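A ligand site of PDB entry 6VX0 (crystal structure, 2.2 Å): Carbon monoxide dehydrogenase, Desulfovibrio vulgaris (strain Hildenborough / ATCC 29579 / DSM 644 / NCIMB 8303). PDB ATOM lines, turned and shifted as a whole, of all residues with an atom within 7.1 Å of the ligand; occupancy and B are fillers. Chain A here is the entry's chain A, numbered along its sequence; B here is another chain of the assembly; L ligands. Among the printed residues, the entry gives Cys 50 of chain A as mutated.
N of Asn 53 lies close to S3 of the ligand (3.8 Å). The guanidinium group of Arg 84 lies close to a sulfur (S2) of the ligand, at 3.6 Å. An iron atom (FE4) of the ligand is bound by the side-chain sulfur (SG) of Cys 54, at 2.3 Å. The side-chain sulfur of Cys 74 is bound to an iron atom (FE3) of the ligand. SG of Cys 59 is bound to FE2 of the ligand (2.3 Å). The side-chain sulfur of Cys 51 binds an iron atom (FE1) of the ligand (2.3 Å). The backbone NH (N) of Cys 74 lies close to a sulfur (S1) of the ligand, at 3.4 Å. N of Cys 54 sits close to S3 of the ligand (3.8 Å).
Residues that only touch the ligand: Met 56 (3.7 Å), Gly 57 (3.8 Å), Gly 72 (3.9 Å), Val 73 (3.8 Å), Ile 81 (3.8 Å) and Met 203 (3.6 Å). Hydrophobic or aromatic side chains that line the ligand: Met 56, Val 73, Ile 81 and Met 203. Of the 29 residues printed, 12 come within 4 Å of the ligand.
The backbone NH of Cys 51 is in hydrogen-bond range of the backbone carbonyl oxygen of Cys 59, at 2.8 Å. SG of Cys 51 sits close to NH2 of Arg 84 (3.4 Å). The backbone carbonyl oxygen (O) of Thr 201 is in hydrogen-bond range of the side-chain amide nitrogen (ND2) of Asn 53, 2.8 Å away. SG of Cys 74 sits close to N of Ala 76 (3.7 Å). The backbone NH (N) of Met 56 lies close to the side-chain sulfur (SG) of Cys 54 (3.4 Å). SG of Cys 51 sits close to N of Asn 53 (3.6 Å). SG of Cys 59 lies close to N of Val 73 (3.5 Å).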
ATOM      1  N   CYS A  50     -16.503  10.845  15.410  1.00  0.00           N
ATOM      2  CA  CYS A  50     -15.892  11.576  14.307  1.00  0.00           C
ATOM      3  C   CYS A  50     -15.745  10.624  13.134  1.00  0.00           C
ATOM      4  O   CYS A  50     -15.278   9.484  13.317  1.00  0.00           O
ATOM      5  CB  CYS A  50     -14.533  12.155  14.689  1.00  0.00           C
ATOM      6  SG  CYS A  50     -13.635  12.955  13.320  1.00  0.00           S
ATOM      7  N   CYS A  51     -16.145  11.065  11.957  1.00  0.00           N
ATOM      8  CA  CYS A  51     -16.066  10.253  10.742  1.00  0.00           C
ATOM      9  C   CYS A  51     -15.256  10.992   9.698  1.00  0.00           C
ATOM     10  O   CYS A  51     -15.447  12.198   9.485  1.00  0.00           O
ATOM     11  CB  CYS A  51     -17.460   9.950  10.198  1.00  0.00           C
ATOM     12  SG  CYS A  51     -17.443   8.855   8.762  1.00  0.00           S
ATOM     13  N   ARG A  52     -14.339  10.264   9.052  1.00  0.00           N
ATOM     14  CA  ARG A  52     -13.442  10.808   8.045  1.00  0.00           C
ATOM     15  C   ARG A  52     -13.471   9.942   6.791  1.00  0.00           C
ATOM     16  O   ARG A  52     -12.474   9.862   6.056  1.00  0.00           O
ATOM     17  CB  ARG A  52     -12.021  10.914   8.588  1.00  0.00           C
ATOM     18  CG  ARG A  52     -11.909  11.731   9.883  1.00  0.00           C
ATOM     19  CD  ARG A  52     -10.508  11.664  10.473  1.00  0.00           C
ATOM     20  NE  ARG A  52     -10.173  10.302  10.900  1.00  0.00           N
ATOM     21  CZ  ARG A  52      -8.991   9.938  11.390  1.00  0.00           C
ATOM     22  NH1 ARG A  52      -8.015  10.825  11.523  1.00  0.00           N
ATOM     23  NH2 ARG A  52      -8.787   8.670  11.750  1.00  0.00           N
ATOM     24  N   ASN A  53     -14.598   9.303   6.525  1.00  0.00           N
ATOM     25  CA  ASN A  53     -14.662   8.292   5.470  1.00  0.00           C
ATOM     26  C   ASN A  53     -14.957   8.880   4.097  1.00  0.00           C
ATOM     27  O   ASN A  53     -14.992   8.120   3.124  1.00  0.00           O
ATOM     28  CB  ASN A  53     -15.715   7.244   5.842  1.00  0.00           C
ATOM     29  CG  ASN A  53     -15.271   6.361   6.993  1.00  0.00           C
ATOM     30  OD1 ASN A  53     -14.316   6.688   7.702  1.00  0.00           O
ATOM     31  ND2 ASN A  53     -15.948   5.231   7.182  1.00  0.00           N
ATOM     32  N   CYS A  54     -15.137  10.188   3.989  1.00  0.00           N
ATOM     33  CA  CYS A  54     -15.247  10.864   2.700  1.00  0.00           C
ATOM     34  C   CYS A  54     -14.980  12.350   2.929  1.00  0.00           C
ATOM     35  O   CYS A  54     -14.948  12.823   4.066  1.00  0.00           O
ATOM     36  CB  CYS A  54     -16.611  10.622   2.046  1.00  0.00           C
ATOM     37  SG  CYS A  54     -17.950  11.681   2.614  1.00  0.00           S
ATOM     38  N   ILE A  55     -14.782  13.085   1.825  1.00  0.00           N
ATOM     39  CA  ILE A  55     -14.472  14.506   1.932  1.00  0.00           C
ATOM     40  C   ILE A  55     -15.707  15.382   1.696  1.00  0.00           C
ATOM     41  O   ILE A  55     -15.569  16.574   1.450  1.00  0.00           O
ATOM     42  CB  ILE A  55     -13.298  14.909   1.015  1.00  0.00           C
ATOM     43  CG1 ILE A  55     -13.681  14.814  -0.461  1.00  0.00           C
ATOM     44  CG2 ILE A  55     -12.056  14.092   1.325  1.00  0.00           C
ATOM     45  CD1 ILE A  55     -12.880  15.759  -1.336  1.00  0.00           C
ATOM     46  N   MET A  56     -16.911  14.805   1.771  1.00  0.00           N
ATOM     47  CA  MET A  56     -18.050  15.626   2.169  1.00  0.00           C
ATOM     48  C   MET A  56     -17.887  16.048   3.621  1.00  0.00           C
ATOM     49  O   MET A  56     -18.325  17.131   4.012  1.00  0.00           O
ATOM     50  CB  MET A  56     -19.370  14.864   1.996  1.00  0.00           C
ATOM     51  CG  MET A  56     -19.770  14.563   0.549  1.00  0.00           C
ATOM     52  SD  MET A  56     -21.542  14.291   0.332  1.00  0.00           S
ATOM     53  CE  MET A  56     -21.838  12.861   1.375  1.00  0.00           C
ATOM     54  N   GLY A  57     -17.245  15.204   4.424  1.00  0.00           N
ATOM     55  CA  GLY A  57     -16.864  15.543   5.762  1.00  0.00           C
ATOM     56  C   GLY A  57     -15.468  16.125   5.810  1.00  0.00           C
ATOM     57  O   GLY A  57     -14.999  16.743   4.850  1.00  0.00           O
ATOM     58  N   PRO A  58     -14.743  15.915   6.931  1.00  0.00           N
ATOM     59  CA  PRO A  58     -15.120  15.093   8.089  1.00  0.00           C
ATOM     60  C   PRO A  58     -16.326  15.604   8.860  1.00  0.00           C
ATOM     61  O   PRO A  58     -16.652  16.786   8.809  1.00  0.00           O
ATOM     62  CB  PRO A  58     -13.856  15.125   8.962  1.00  0.00           C
ATOM     63  CG  PRO A  58     -13.151  16.377   8.567  1.00  0.00           C
ATOM     64  CD  PRO A  58     -13.415  16.537   7.108  1.00  0.00           C
ATOM     65  N   CYS A  59     -17.010  14.700   9.540  1.00  0.00           N
ATOM     66  CA  CYS A  59     -18.207  15.022  10.300  1.00  0.00           C
ATOM     67  C   CYS A  59     -18.021  14.560  11.734  1.00  0.00           C
ATOM     68  O   CYS A  59     -17.419  13.514  11.992  1.00  0.00           O
ATOM     69  CB  CYS A  59     -19.453  14.354   9.709  1.00  0.00           C
ATOM     70  SG  CYS A  59     -19.660  14.621   7.943  1.00  0.00           S
ATOM     71  N   ARG A  60     -18.536  15.345  12.675  1.00  0.00           N
ATOM     72  CA  ARG A  60     -18.611  14.932  14.061  1.00  0.00           C
ATOM     73  C   ARG A  60     -20.054  15.024  14.536  1.00  0.00           C
ATOM     74  O   ARG A  60     -20.759  15.984  14.208  1.00  0.00           O
ATOM     75  CB  ARG A  60     -17.687  15.763  14.964  1.00  0.00           C
ATOM     76  CG  ARG A  60     -17.721  17.248  14.713  1.00  0.00           C
ATOM     77  N   ILE A  61     -20.489  14.016  15.275  1.00  0.00           N
ATOM     78  CA  ILE A  61     -21.815  13.999  15.869  1.00  0.00           C
ATOM     79  C   ILE A  61     -21.675  14.537  17.289  1.00  0.00           C
ATOM     80  O   ILE A  61     -20.895  14.008  18.089  1.00  0.00           O
ATOM     81  CB  ILE A  61     -22.428  12.595  15.864  1.00  0.00           C
ATOM     82  CG1 ILE A  61     -22.389  12.015  14.455  1.00  0.00           C
ATOM     83  CG2 ILE A  61     -23.854  12.651  16.360  1.00  0.00           C
ATOM     84  CD1 ILE A  61     -23.101  12.863  13.418  1.00  0.00           C
ATOM     85  N   LEU A  71     -26.370  14.693  12.615  1.00  0.00           N
ATOM     86  CA  LEU A  71     -26.137  13.766  11.517  1.00  0.00           C
ATOM     87  C   LEU A  71     -24.940  14.224  10.699  1.00  0.00           C
ATOM     88  O   LEU A  71     -24.610  15.409  10.643  1.00  0.00           O
ATOM     89  CB  LEU A  71     -27.370  13.668  10.614  1.00  0.00           C
ATOM     90  CG  LEU A  71     -28.685  13.285  11.304  1.00  0.00           C
ATOM     91  CD1 LEU A  71     -29.851  13.405  10.334  1.00  0.00           C
ATOM     92  CD2 LEU A  71     -28.600  11.871  11.864  1.00  0.00           C
ATOM     93  N   GLY A  72     -24.280  13.260  10.047  1.00  0.00           N
ATOM     94  CA  GLY A  72     -23.261  13.587   9.080  1.00  0.00           C
ATOM     95  C   GLY A  72     -23.873  14.146   7.812  1.00  0.00           C
ATOM     96  O   GLY A  72     -25.094  14.146   7.612  1.00  0.00           O
ATOM     97  N   VAL A  73     -23.010  14.642   6.922  1.00  0.00           N
ATOM     98  CA  VAL A  73     -23.481  15.244   5.686  1.00  0.00           C
ATOM     99  C   VAL A  73     -24.294  14.243   4.872  1.00  0.00           C
ATOM    100  O   VAL A  73     -25.307  14.599   4.243  1.00  0.00           O
ATOM    101  CB  VAL A  73     -22.295  15.816   4.887  1.00  0.00           C
ATOM    102  CG1 VAL A  73     -22.776  16.430   3.576  1.00  0.00           C
ATOM    103  CG2 VAL A  73     -21.546  16.857   5.715  1.00  0.00           C
ATOM    104  N   CYS A  74     -23.897  12.978   4.886  1.00  0.00           N
ATOM    105  CA  CYS A  74     -24.657  11.935   4.194  1.00  0.00           C
ATOM    106  C   CYS A  74     -25.919  11.520   4.939  1.00  0.00           C
ATOM    107  O   CYS A  74     -26.751  10.799   4.377  1.00  0.00           O
ATOM    108  CB  CYS A  74     -23.780  10.697   3.963  1.00  0.00           C
ATOM    109  SG  CYS A  74     -23.174   9.907   5.489  1.00  0.00           S
ATOM    110  N   GLY A  75     -26.083  11.949   6.188  1.00  0.00           N
ATOM    111  CA  GLY A  75     -27.227  11.559   6.992  1.00  0.00           C
ATOM    112  C   GLY A  75     -26.945  10.520   8.050  1.00  0.00           C
ATOM    113  O   GLY A  75     -27.843  10.212   8.840  1.00  0.00           O
ATOM    114  N   ALA A  76     -25.719   9.990   8.120  1.00  0.00           N
ATOM    115  CA  ALA A  76     -25.395   8.972   9.095  1.00  0.00           C
ATOM    116  C   ALA A  76     -25.433   9.541  10.513  1.00  0.00           C
ATOM    117  O   ALA A  76     -25.017  10.679  10.750  1.00  0.00           O
ATOM    118  CB  ALA A  76     -24.013   8.375   8.816  1.00  0.00           C
ATOM    119  N   ASP A  77     -25.963   8.758  11.447  1.00  0.00           N
ATOM    120  CA  ASP A  77     -26.086   9.166  12.835  1.00  0.00           C
ATOM    121  C   ASP A  77     -24.943   8.590  13.669  1.00  0.00           C
ATOM    122  O   ASP A  77     -24.034   7.923  13.158  1.00  0.00           O
ATOM    123  CB  ASP A  77     -27.459   8.760  13.403  1.00  0.00           C
ATOM    124  CG  ASP A  77     -27.675   7.252  13.423  1.00  0.00           C
ATOM    125  OD1 ASP A  77     -26.711   6.469  13.237  1.00  0.00           O
ATOM    126  OD2 ASP A  77     -28.836   6.833  13.622  1.00  0.00           O
ATOM    127  N   ILE A  81     -21.942   5.809  12.678  1.00  0.00           N
ATOM    128  CA  ILE A  81     -20.576   6.314  12.623  1.00  0.00           C
ATOM    129  C   ILE A  81     -19.690   5.586  13.637  1.00  0.00           C
ATOM    130  O   ILE A  81     -18.556   5.188  13.316  1.00  0.00           O
ATOM    131  CB  ILE A  81     -20.560   7.838  12.836  1.00  0.00           C
ATOM    132  CG1 ILE A  81     -21.100   8.542  11.591  1.00  0.00           C
ATOM    133  CG2 ILE A  81     -19.149   8.333  13.150  1.00  0.00           C
ATOM    134  CD1 ILE A  81     -21.247  10.035  11.733  1.00  0.00           C
ATOM    135  N   ARG A  84     -19.213   1.898  12.430  1.00  0.00           N
ATOM    136  CA  ARG A  84     -18.272   1.781  11.316  1.00  0.00           C
ATOM    137  C   ARG A  84     -16.834   1.960  11.788  1.00  0.00           C
ATOM    138  O   ARG A  84     -15.948   1.207  11.378  1.00  0.00           O
ATOM    139  CB  ARG A  84     -18.622   2.798  10.229  1.00  0.00           C
ATOM    140  CG  ARG A  84     -19.896   2.485   9.461  1.00  0.00           C
ATOM    141  CD  ARG A  84     -20.058   3.380   8.238  1.00  0.00           C
ATOM    142  NE  ARG A  84     -19.928   4.798   8.540  1.00  0.00           N
ATOM    143  CZ  ARG A  84     -20.440   5.771   7.800  1.00  0.00           C
ATOM    144  NH1 ARG A  84     -21.139   5.477   6.716  1.00  0.00           N
ATOM    145  NH2 ARG A  84     -20.265   7.041   8.149  1.00  0.00           N
ATOM    146  N   THR A 201     -18.097  -0.223   5.517  1.00  0.00           N
ATOM    147  CA  THR A 201     -17.881   1.041   6.205  1.00  0.00           C
ATOM    148  C   THR A 201     -17.633   2.206   5.259  1.00  0.00           C
ATOM    149  O   THR A 201     -17.437   3.339   5.729  1.00  0.00           O
ATOM    150  CB  THR A 201     -16.720   0.877   7.201  1.00  0.00           C
ATOM    151  OG1 THR A 201     -15.543   0.418   6.512  1.00  0.00           O
ATOM    152  CG2 THR A 201     -17.112  -0.140   8.265  1.00  0.00           C
ATOM    153  N   HIS A 202     -17.591   1.958   3.947  1.00  0.00           N
ATOM    154  CA  HIS A 202     -17.593   3.026   2.974  1.00  0.00           C
ATOM    155  C   HIS A 202     -18.906   3.794   3.069  1.00  0.00           C
ATOM    156  O   HIS A 202     -19.938   3.243   3.471  1.00  0.00           O
ATOM    157  CB  HIS A 202     -17.418   2.428   1.567  1.00  0.00           C
ATOM    158  CG  HIS A 202     -17.350   3.445   0.473  1.00  0.00           C
ATOM    159  ND1 HIS A 202     -16.171   3.789  -0.154  1.00  0.00           N
ATOM    160  CD2 HIS A 202     -18.316   4.179  -0.121  1.00  0.00           C
ATOM    161  CE1 HIS A 202     -16.411   4.701  -1.082  1.00  0.00           C
ATOM    162  NE2 HIS A 202     -17.715   4.955  -1.087  1.00  0.00           N
ATOM    163  N   MET A 203     -18.869   5.090   2.730  1.00  0.00           N
ATOM    164  CA  MET A 203     -20.075   5.906   2.744  1.00  0.00           C
ATOM    165  C   MET A 203     -21.205   5.223   1.978  1.00  0.00           C
ATOM    166  O   MET A 203     -21.003   4.698   0.877  1.00  0.00           O
ATOM    167  CB  MET A 203     -19.799   7.288   2.122  1.00  0.00           C
ATOM    168  CG  MET A 203     -20.945   8.315   2.220  1.00  0.00           C
ATOM    169  SD  MET A 203     -22.440   8.009   1.221  1.00  0.00           S
ATOM    170  CE  MET A 203     -22.566   9.489   0.214  1.00  0.00           C
ATOM    171  N   GLY A 204     -22.388   5.227   2.577  1.00  0.00           N
ATOM    172  CA  GLY A 204     -23.561   4.773   1.878  1.00  0.00           C
ATOM    173  C   GLY A 204     -23.618   3.288   1.595  1.00  0.00           C
ATOM    174  O   GLY A 204     -24.303   2.883   0.643  1.00  0.00           O
ATOM    175  N   ASN A 207     -25.412   0.893   6.745  1.00  0.00           N
ATOM    176  CA  ASN A 207     -25.840   1.955   7.644  1.00  0.00           C
ATOM    177  C   ASN A 207     -26.807   1.425   8.702  1.00  0.00           C
ATOM    178  O   ASN A 207     -27.861   2.021   8.940  1.00  0.00           O
ATOM    179  CB  ASN A 207     -26.482   3.087   6.850  1.00  0.00           C
ATOM    180  CG  ASN A 207     -25.476   3.844   6.015  1.00  0.00           C
ATOM    181  OD1 ASN A 207     -25.017   4.920   6.396  1.00  0.00           O
ATOM    182  ND2 ASN A 207     -25.127   3.282   4.855  1.00  0.00           N
ATOM    183  N   GLN B  38     -21.827  20.963   9.324  1.00  0.00           N
ATOM    184  CA  GLN B  38     -20.575  20.253   9.550  1.00  0.00           C
ATOM    185  C   GLN B  38     -19.341  21.023   9.096  1.00  0.00           C
ATOM    186  O   GLN B  38     -18.237  20.472   9.135  1.00  0.00           O
ATOM    187  CB  GLN B  38     -20.601  18.893   8.861  1.00  0.00           C
ATOM    188  CG  GLN B  38     -21.567  17.874   9.474  1.00  0.00           C
ATOM    189  CD  GLN B  38     -21.148  17.441  10.862  1.00  0.00           C
ATOM    190  OE1 GLN B  38     -20.008  17.644  11.283  1.00  0.00           O
ATOM    191  NE2 GLN B  38     -22.082  16.822  11.597  1.00  0.00           N
ATOM    192  N   PRO B 343     -28.053   7.603   3.789  1.00  0.00           N
ATOM    193  CA  PRO B 343     -29.132   7.143   4.677  1.00  0.00           C
ATOM    194  C   PRO B 343     -30.189   8.199   4.959  1.00  0.00           C
ATOM    195  O   PRO B 343     -31.240   7.854   5.520  1.00  0.00           O
ATOM    196  CB  PRO B 343     -28.387   6.748   5.960  1.00  0.00           C
ATOM    197  CG  PRO B 343     -27.089   7.508   5.906  1.00  0.00           C
ATOM    198  CD  PRO B 343     -26.740   7.595   4.444  1.00  0.00           C
ATOM    199  N   TYR B 553     -15.936  13.120  -3.898  1.00  0.00           N
ATOM    200  CA  TYR B 553     -16.042  13.040  -2.442  1.00  0.00           C
ATOM    201  C   TYR B 553     -15.662  11.683  -1.856  1.00  0.00           C
ATOM    202  O   TYR B 553     -15.170  11.647  -0.721  1.00  0.00           O
ATOM    203  CB  TYR B 553     -17.473  13.381  -1.987  1.00  0.00           C
ATOM    204  CG  TYR B 553     -18.448  12.224  -2.116  1.00  0.00           C
ATOM    205  CD1 TYR B 553     -19.133  12.006  -3.300  1.00  0.00           C
ATOM    206  CD2 TYR B 553     -18.639  11.331  -1.064  1.00  0.00           C
ATOM    207  CE1 TYR B 553     -19.998  10.941  -3.423  1.00  0.00           C
ATOM    208  CE2 TYR B 553     -19.488  10.270  -1.184  1.00  0.00           C
ATOM    209  CZ  TYR B 553     -20.175  10.081  -2.365  1.00  0.00           C
ATOM    210  OH  TYR B 553     -21.027   9.014  -2.492  1.00  0.00           O
HETATM  211 FE1  LIG L   1     -18.623  10.046   7.235  1.00  0.00          FE
HETATM  212 FE2  LIG L   1     -19.543  12.592   6.903  1.00  0.00          FE
HETATM  213 FE3  LIG L   1     -21.013  10.478   5.955  1.00  0.00          FE
HETATM  214 FE4  LIG L   1     -18.640  11.163   4.739  1.00  0.00          FE
HETATM  215  S1  LIG L   1     -20.547  12.425   4.861  1.00  0.00           S
HETATM  216  S2  LIG L   1     -19.333   9.061   5.318  1.00  0.00           S
HETATM  217  S3  LIG L   1     -17.417  11.843   6.536  1.00  0.00           S
HETATM  218  S4  LIG L   1     -20.518  10.945   8.132  1.00  0.00           S
